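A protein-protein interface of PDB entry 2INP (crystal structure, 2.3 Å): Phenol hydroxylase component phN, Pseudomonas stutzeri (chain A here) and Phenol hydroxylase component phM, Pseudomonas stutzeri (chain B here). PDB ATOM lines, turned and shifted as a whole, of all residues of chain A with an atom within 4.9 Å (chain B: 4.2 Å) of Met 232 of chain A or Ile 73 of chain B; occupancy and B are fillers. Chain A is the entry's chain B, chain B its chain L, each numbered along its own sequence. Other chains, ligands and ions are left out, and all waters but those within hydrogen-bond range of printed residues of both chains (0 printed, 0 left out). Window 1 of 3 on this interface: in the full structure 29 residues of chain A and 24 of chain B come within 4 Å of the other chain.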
ATOM      1  N   GLU A 194      25.522   4.639 -22.782  1.00  0.00           N
ATOM      2  CA  GLU A 194      25.363   3.248 -22.340  1.00  0.00           C
ATOM      3  C   GLU A 194      23.992   2.609 -22.662  1.00  0.00           C
ATOM      4  O   GLU A 194      23.900   1.392 -22.619  1.00  0.00           O
ATOM      5  CB  GLU A 194      25.768   3.025 -20.859  1.00  0.00           C
ATOM      6  CG  GLU A 194      27.103   2.230 -20.775  1.00  0.00           C
ATOM      7  CD  GLU A 194      27.867   2.452 -19.523  1.00  0.00           C
ATOM      8  OE1 GLU A 194      28.671   1.549 -19.065  1.00  0.00           O
ATOM      9  OE2 GLU A 194      27.658   3.566 -18.997  1.00  0.00           O
ATOM     10  N   TYR A 195      22.966   3.405 -23.002  1.00  0.00           N
ATOM     11  CA  TYR A 195      21.632   2.903 -23.350  1.00  0.00           C
ATOM     12  C   TYR A 195      21.311   3.146 -24.831  1.00  0.00           C
ATOM     13  O   TYR A 195      21.194   2.171 -25.595  1.00  0.00           O
ATOM     14  CB  TYR A 195      20.536   3.516 -22.457  1.00  0.00           C
ATOM     15  CG  TYR A 195      19.153   2.959 -22.776  1.00  0.00           C
ATOM     16  CD1 TYR A 195      18.144   3.766 -23.359  1.00  0.00           C
ATOM     17  CD2 TYR A 195      18.858   1.617 -22.518  1.00  0.00           C
ATOM     18  CE1 TYR A 195      16.891   3.240 -23.643  1.00  0.00           C
ATOM     19  CE2 TYR A 195      17.676   1.087 -22.811  1.00  0.00           C
ATOM     20  CZ  TYR A 195      16.677   1.885 -23.376  1.00  0.00           C
ATOM     21  OH  TYR A 195      15.469   1.274 -23.667  1.00  0.00           O
ATOM     22  N   THR A 198      24.659   2.244 -27.181  1.00  0.00           N
ATOM     23  CA  THR A 198      25.556   1.218 -26.653  1.00  0.00           C
ATOM     24  C   THR A 198      25.841   0.116 -27.694  1.00  0.00           C
ATOM     25  O   THR A 198      26.977  -0.349 -27.851  1.00  0.00           O
ATOM     26  CB  THR A 198      24.956   0.669 -25.337  1.00  0.00           C
ATOM     27  OG1 THR A 198      25.888  -0.221 -24.701  1.00  0.00           O
ATOM     28  CG2 THR A 198      23.607   0.052 -25.551  1.00  0.00           C
ATOM     29  N   ASN A 199      24.797  -0.199 -28.454  1.00  0.00           N
ATOM     30  CA  ASN A 199      24.817  -1.207 -29.450  1.00  0.00           C
ATOM     31  C   ASN A 199      25.575  -0.765 -30.684  1.00  0.00           C
ATOM     32  O   ASN A 199      26.140  -1.597 -31.372  1.00  0.00           O
ATOM     33  CB  ASN A 199      23.367  -1.533 -29.835  1.00  0.00           C
ATOM     34  CG  ASN A 199      22.602  -2.314 -28.738  1.00  0.00           C
ATOM     35  OD1 ASN A 199      23.076  -2.509 -27.560  1.00  0.00           O
ATOM     36  ND2 ASN A 199      21.401  -2.756 -29.119  1.00  0.00           N
ATOM     37  N   GLU A 228      26.222  -5.166 -19.137  1.00  0.00           N
ATOM     38  CA  GLU A 228      25.546  -4.174 -19.977  1.00  0.00           C
ATOM     39  C   GLU A 228      24.033  -4.112 -19.724  1.00  0.00           C
ATOM     40  O   GLU A 228      23.430  -3.037 -19.660  1.00  0.00           O
ATOM     41  CB  GLU A 228      25.833  -4.467 -21.470  1.00  0.00           C
ATOM     42  CG  GLU A 228      27.135  -3.878 -21.916  1.00  0.00           C
ATOM     43  CD  GLU A 228      27.543  -2.605 -21.157  1.00  0.00           C
ATOM     44  OE1 GLU A 228      26.823  -1.609 -21.081  1.00  0.00           O
ATOM     45  OE2 GLU A 228      28.662  -2.595 -20.650  1.00  0.00           O
ATOM     46  N   ALA A 229      23.424  -5.270 -19.592  1.00  0.00           N
ATOM     47  CA  ALA A 229      22.044  -5.279 -19.200  1.00  0.00           C
ATOM     48  C   ALA A 229      21.840  -4.367 -17.992  1.00  0.00           C
ATOM     49  O   ALA A 229      20.896  -3.565 -18.002  1.00  0.00           O
ATOM     50  CB  ALA A 229      21.555  -6.715 -18.931  1.00  0.00           C
ATOM     51  N   ARG A 230      22.718  -4.449 -16.981  1.00  0.00           N
ATOM     52  CA  ARG A 230      22.521  -3.662 -15.732  1.00  0.00           C
ATOM     53  C   ARG A 230      22.790  -2.196 -16.004  1.00  0.00           C
ATOM     54  O   ARG A 230      22.157  -1.295 -15.422  1.00  0.00           O
ATOM     55  CB  ARG A 230      23.395  -4.152 -14.576  1.00  0.00           C
ATOM     56  CG  ARG A 230      23.034  -5.531 -13.962  1.00  0.00           C
ATOM     57  CD  ARG A 230      23.775  -5.657 -12.595  1.00  0.00           C
ATOM     58  NE  ARG A 230      25.240  -5.420 -12.739  1.00  0.00           N
ATOM     59  CZ  ARG A 230      26.127  -6.328 -13.144  1.00  0.00           C
ATOM     60  NH1 ARG A 230      25.726  -7.585 -13.430  1.00  0.00           N
ATOM     61  NH2 ARG A 230      27.399  -5.981 -13.294  1.00  0.00           N
ATOM     62  N   HIS A 231      23.763  -1.974 -16.879  1.00  0.00           N
ATOM     63  CA  HIS A 231      24.212  -0.664 -17.292  1.00  0.00           C
ATOM     64  C   HIS A 231      23.104   0.112 -18.115  1.00  0.00           C
ATOM     65  O   HIS A 231      22.873   1.302 -17.944  1.00  0.00           O
ATOM     66  CB  HIS A 231      25.573  -0.870 -18.001  1.00  0.00           C
ATOM     67  CG  HIS A 231      26.680  -1.307 -17.054  1.00  0.00           C
ATOM     68  ND1 HIS A 231      28.016  -1.349 -17.412  1.00  0.00           N
ATOM     69  CD2 HIS A 231      26.643  -1.689 -15.751  1.00  0.00           C
ATOM     70  CE1 HIS A 231      28.748  -1.746 -16.384  1.00  0.00           C
ATOM     71  NE2 HIS A 231      27.937  -1.969 -15.364  1.00  0.00           N
ATOM     72  N   MET A 232      22.384  -0.591 -18.977  1.00  0.00           N
ATOM     73  CA  MET A 232      21.224  -0.016 -19.658  1.00  0.00           C
ATOM     74  C   MET A 232      20.128   0.406 -18.666  1.00  0.00           C
ATOM     75  O   MET A 232      19.511   1.484 -18.814  1.00  0.00           O
ATOM     76  CB  MET A 232      20.681  -1.029 -20.645  1.00  0.00           C
ATOM     77  CG  MET A 232      21.645  -1.134 -21.720  1.00  0.00           C
ATOM     78  SD  MET A 232      21.468  -2.349 -22.996  1.00  0.00           S
ATOM     79  CE  MET A 232      20.412  -1.496 -24.273  1.00  0.00           C
ATOM     80  N   THR A 233      19.916  -0.436 -17.648  1.00  0.00           N
ATOM     81  CA  THR A 233      18.821  -0.266 -16.726  1.00  0.00           C
ATOM     82  C   THR A 233      19.027   0.939 -15.856  1.00  0.00           C
ATOM     83  O   THR A 233      18.083   1.653 -15.599  1.00  0.00           O
ATOM     84  CB  THR A 233      18.651  -1.509 -15.859  1.00  0.00           C
ATOM     85  OG1 THR A 233      18.330  -2.608 -16.704  1.00  0.00           O
ATOM     86  CG2 THR A 233      17.538  -1.328 -14.981  1.00  0.00           C
ATOM     87  N   LEU A 234      20.244   1.155 -15.373  1.00  0.00           N
ATOM     88  CA  LEU A 234      20.533   2.396 -14.683  1.00  0.00           C
ATOM     89  C   LEU A 234      20.302   3.647 -15.614  1.00  0.00           C
ATOM     90  O   LEU A 234      19.747   4.646 -15.186  1.00  0.00           O
ATOM     91  CB  LEU A 234      21.924   2.358 -14.073  1.00  0.00           C
ATOM     92  CG  LEU A 234      22.481   3.637 -13.454  1.00  0.00           C
ATOM     93  CD1 LEU A 234      21.731   4.085 -12.221  1.00  0.00           C
ATOM     94  CD2 LEU A 234      23.991   3.530 -13.130  1.00  0.00           C
ATOM     95  N   GLY A 235      20.693   3.564 -16.882  1.00  0.00           N
ATOM     96  CA  GLY A 235      20.482   4.671 -17.800  1.00  0.00           C
ATOM     97  C   GLY A 235      19.022   5.039 -18.013  1.00  0.00           C
ATOM     98  O   GLY A 235      18.690   6.221 -18.020  1.00  0.00           O
ATOM     99  N   LEU A 236      18.156   4.041 -18.184  1.00  0.00           N
ATOM    100  CA  LEU A 236      16.740   4.292 -18.266  1.00  0.00           C
ATOM    101  C   LEU A 236      16.157   4.731 -16.917  1.00  0.00           C
ATOM    102  O   LEU A 236      15.388   5.678 -16.868  1.00  0.00           O
ATOM    103  CB  LEU A 236      16.042   3.074 -18.758  1.00  0.00           C
ATOM    104  CG  LEU A 236      15.169   3.236 -19.984  1.00  0.00           C
ATOM    105  CD1 LEU A 236      14.343   1.966 -20.057  1.00  0.00           C
ATOM    106  CD2 LEU A 236      14.258   4.499 -19.972  1.00  0.00           C
ATOM    107  N   PHE B   6      14.472  -6.362 -26.044  1.00  0.00           N
ATOM    108  CA  PHE B   6      15.388  -7.361 -26.504  1.00  0.00           C
ATOM    109  C   PHE B   6      16.396  -7.825 -25.480  1.00  0.00           C
ATOM    110  O   PHE B   6      16.694  -7.148 -24.502  1.00  0.00           O
ATOM    111  CB  PHE B   6      16.051  -6.941 -27.837  1.00  0.00           C
ATOM    112  CG  PHE B   6      17.139  -5.893 -27.697  1.00  0.00           C
ATOM    113  CD1 PHE B   6      18.332  -6.176 -27.011  1.00  0.00           C
ATOM    114  CD2 PHE B   6      17.002  -4.651 -28.305  1.00  0.00           C
ATOM    115  CE1 PHE B   6      19.341  -5.219 -26.889  1.00  0.00           C
ATOM    116  CE2 PHE B   6      18.018  -3.682 -28.196  1.00  0.00           C
ATOM    117  CZ  PHE B   6      19.174  -3.969 -27.478  1.00  0.00           C
ATOM    118  N   ILE B   7      16.906  -9.016 -25.764  1.00  0.00           N
ATOM    119  CA  ILE B   7      17.851  -9.731 -24.940  1.00  0.00           C
ATOM    120  C   ILE B   7      18.734 -10.548 -25.904  1.00  0.00           C
ATOM    121  O   ILE B   7      18.236 -11.270 -26.765  1.00  0.00           O
ATOM    122  CB  ILE B   7      17.106 -10.602 -23.846  1.00  0.00           C
ATOM    123  CG1 ILE B   7      18.079 -11.133 -22.769  1.00  0.00           C
ATOM    124  CG2 ILE B   7      16.240 -11.733 -24.480  1.00  0.00           C
ATOM    125  CD1 ILE B   7      17.418 -11.399 -21.419  1.00  0.00           C
ATOM    126  N   SER B  72      23.780  -7.714 -23.618  1.00  0.00           N
ATOM    127  CA  SER B  72      22.848  -6.614 -23.765  1.00  0.00           C
ATOM    128  C   SER B  72      21.421  -6.969 -23.334  1.00  0.00           C
ATOM    129  O   SER B  72      21.113  -8.112 -22.981  1.00  0.00           O
ATOM    130  CB  SER B  72      22.852  -6.100 -25.211  1.00  0.00           C
ATOM    131  OG  SER B  72      22.262  -7.054 -26.098  1.00  0.00           O
ATOM    132  N   ILE B  73      20.557  -5.959 -23.376  1.00  0.00           N
ATOM    133  CA  ILE B  73      19.161  -6.066 -22.964  1.00  0.00           C
ATOM    134  C   ILE B  73      18.409  -4.864 -23.554  1.00  0.00           C
ATOM    135  O   ILE B  73      19.015  -4.010 -24.191  1.00  0.00           O
ATOM    136  CB  ILE B  73      19.051  -6.157 -21.414  1.00  0.00           C
ATOM    137  CG1 ILE B  73      18.281  -7.430 -21.007  1.00  0.00           C
ATOM    138  CG2 ILE B  73      18.630  -4.805 -20.752  1.00  0.00           C
ATOM    139  CD1 ILE B  73      17.884  -7.545 -19.492  1.00  0.00           C
ATOM    140  N   ALA B  74      17.099  -4.786 -23.387  1.00  0.00           N
ATOM    141  CA  ALA B  74      16.387  -3.592 -23.859  1.00  0.00           C
ATOM    142  C   ALA B  74      14.984  -3.465 -23.273  1.00  0.00           C
ATOM    143  O   ALA B  74      14.211  -4.432 -23.228  1.00  0.00           O
ATOM    144  CB  ALA B  74      16.362  -3.522 -25.397  1.00  0.00           C
ATOM    145  N   VAL B  77      13.367  -2.945 -16.812  1.00  0.00           N
ATOM    146  CA  VAL B  77      13.633  -4.213 -16.134  1.00  0.00           C
ATOM    147  C   VAL B  77      12.697  -4.491 -14.969  1.00  0.00           C
ATOM    148  O   VAL B  77      12.543  -3.664 -14.064  1.00  0.00           O
ATOM    149  CB  VAL B  77      15.137  -4.395 -15.762  1.00  0.00           C
ATOM    150  CG1 VAL B  77      15.343  -5.381 -14.593  1.00  0.00           C
ATOM    151  CG2 VAL B  77      15.922  -4.862 -17.000  1.00  0.00           C
ATOM    152  N   PHE B  84      11.886 -12.557 -14.665  1.00  0.00           N
ATOM    153  CA  PHE B  84      12.671 -11.530 -15.340  1.00  0.00           C
ATOM    154  C   PHE B  84      11.965 -11.080 -16.636  1.00  0.00           C
ATOM    155  O   PHE B  84      11.802 -11.852 -17.576  1.00  0.00           O
ATOM    156  CB  PHE B  84      14.106 -12.003 -15.602  1.00  0.00           C
ATOM    157  CG  PHE B  84      15.065 -10.880 -15.888  1.00  0.00           C
ATOM    158  CD1 PHE B  84      16.003 -10.503 -14.942  1.00  0.00           C
ATOM    159  CD2 PHE B  84      15.004 -10.180 -17.090  1.00  0.00           C
ATOM    160  CE1 PHE B  84      16.885  -9.469 -15.198  1.00  0.00           C
ATOM    161  CE2 PHE B  84      15.857  -9.148 -17.348  1.00  0.00           C
ATOM    162  CZ  PHE B  84      16.811  -8.783 -16.398  1.00  0.00           C
ATOM    163  N   LEU B  86      11.403  -7.924 -19.669  1.00  0.00           N
ATOM    164  CA  LEU B  86      11.747  -6.674 -20.352  1.00  0.00           C
ATOM    165  C   LEU B  86      10.475  -6.033 -20.965  1.00  0.00           C
ATOM    166  O   LEU B  86       9.717  -6.707 -21.681  1.00  0.00           O
ATOM    167  CB  LEU B  86      12.837  -6.930 -21.411  1.00  0.00           C
ATOM    168  CG  LEU B  86      14.272  -7.083 -20.883  1.00  0.00           C
ATOM    169  CD1 LEU B  86      15.132  -7.896 -21.823  1.00  0.00           C
ATOM    170  CD2 LEU B  86      14.918  -5.722 -20.606  1.00  0.00           C
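Of the 13 printed residues of chain A, 4 touch a printed residue of chain B. Of the 8 printed residues of chain B, 3 touch a printed residue of chain A. Hydrophobic or aromatic side chains of chain B within 4 Å of the printed part of chain A: Phe 6, Ile 73 and Val 77. Along chain B the printed residues that touch a printed residue of chain A span positions 6 to 77. Among the printed residues, 4 pairs touch across the chains.
Printed residues of chain B within 4 Å of Ala 229 of chain A: Ile 73. Met 232 of chain A touches just one residue of chain B: Ile 73. Of the printed residues of chain B, Thr 233 of chain A touches Val 77. Ser 72 of chain B touches none of the printed residues of chain A. Ile 73 of chain B touches just these residues of chain A: Ala 229 and Met 232. Printed residues of chain A within 4 Å of Val 77 of chain B: Thr 233 (3.3 Å). The nearest printed residue of chain B that does not touch Met 232 of chain A is Phe 6 of chain B (4.2 Å).
Among the printed residues, pairs that only touch across the chains: Asn 199 of chain A with Phe 6 of chain B (3.0 Å), Ala 229 of chain A with Ile 73 of chain B (3.6 Å) and Thr 233 of chain A with Val 77 of chain B (3.3 Å).
SD of Met 232 of chain A sits at hydrogen-bond distance from N of Ile 73 of chain B, 3.7 Å away.
O of Ala 229 of chain A sits at hydrogen-bond distance from OG1 of Thr 233 of chain A, at 3.0 Å. The backbone carbonyl oxygen (O) of Phe 6 of chain B lies within hydrogen-bond range of the backbone NH (N) of Ala 74 of chain B (2.6 Å).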
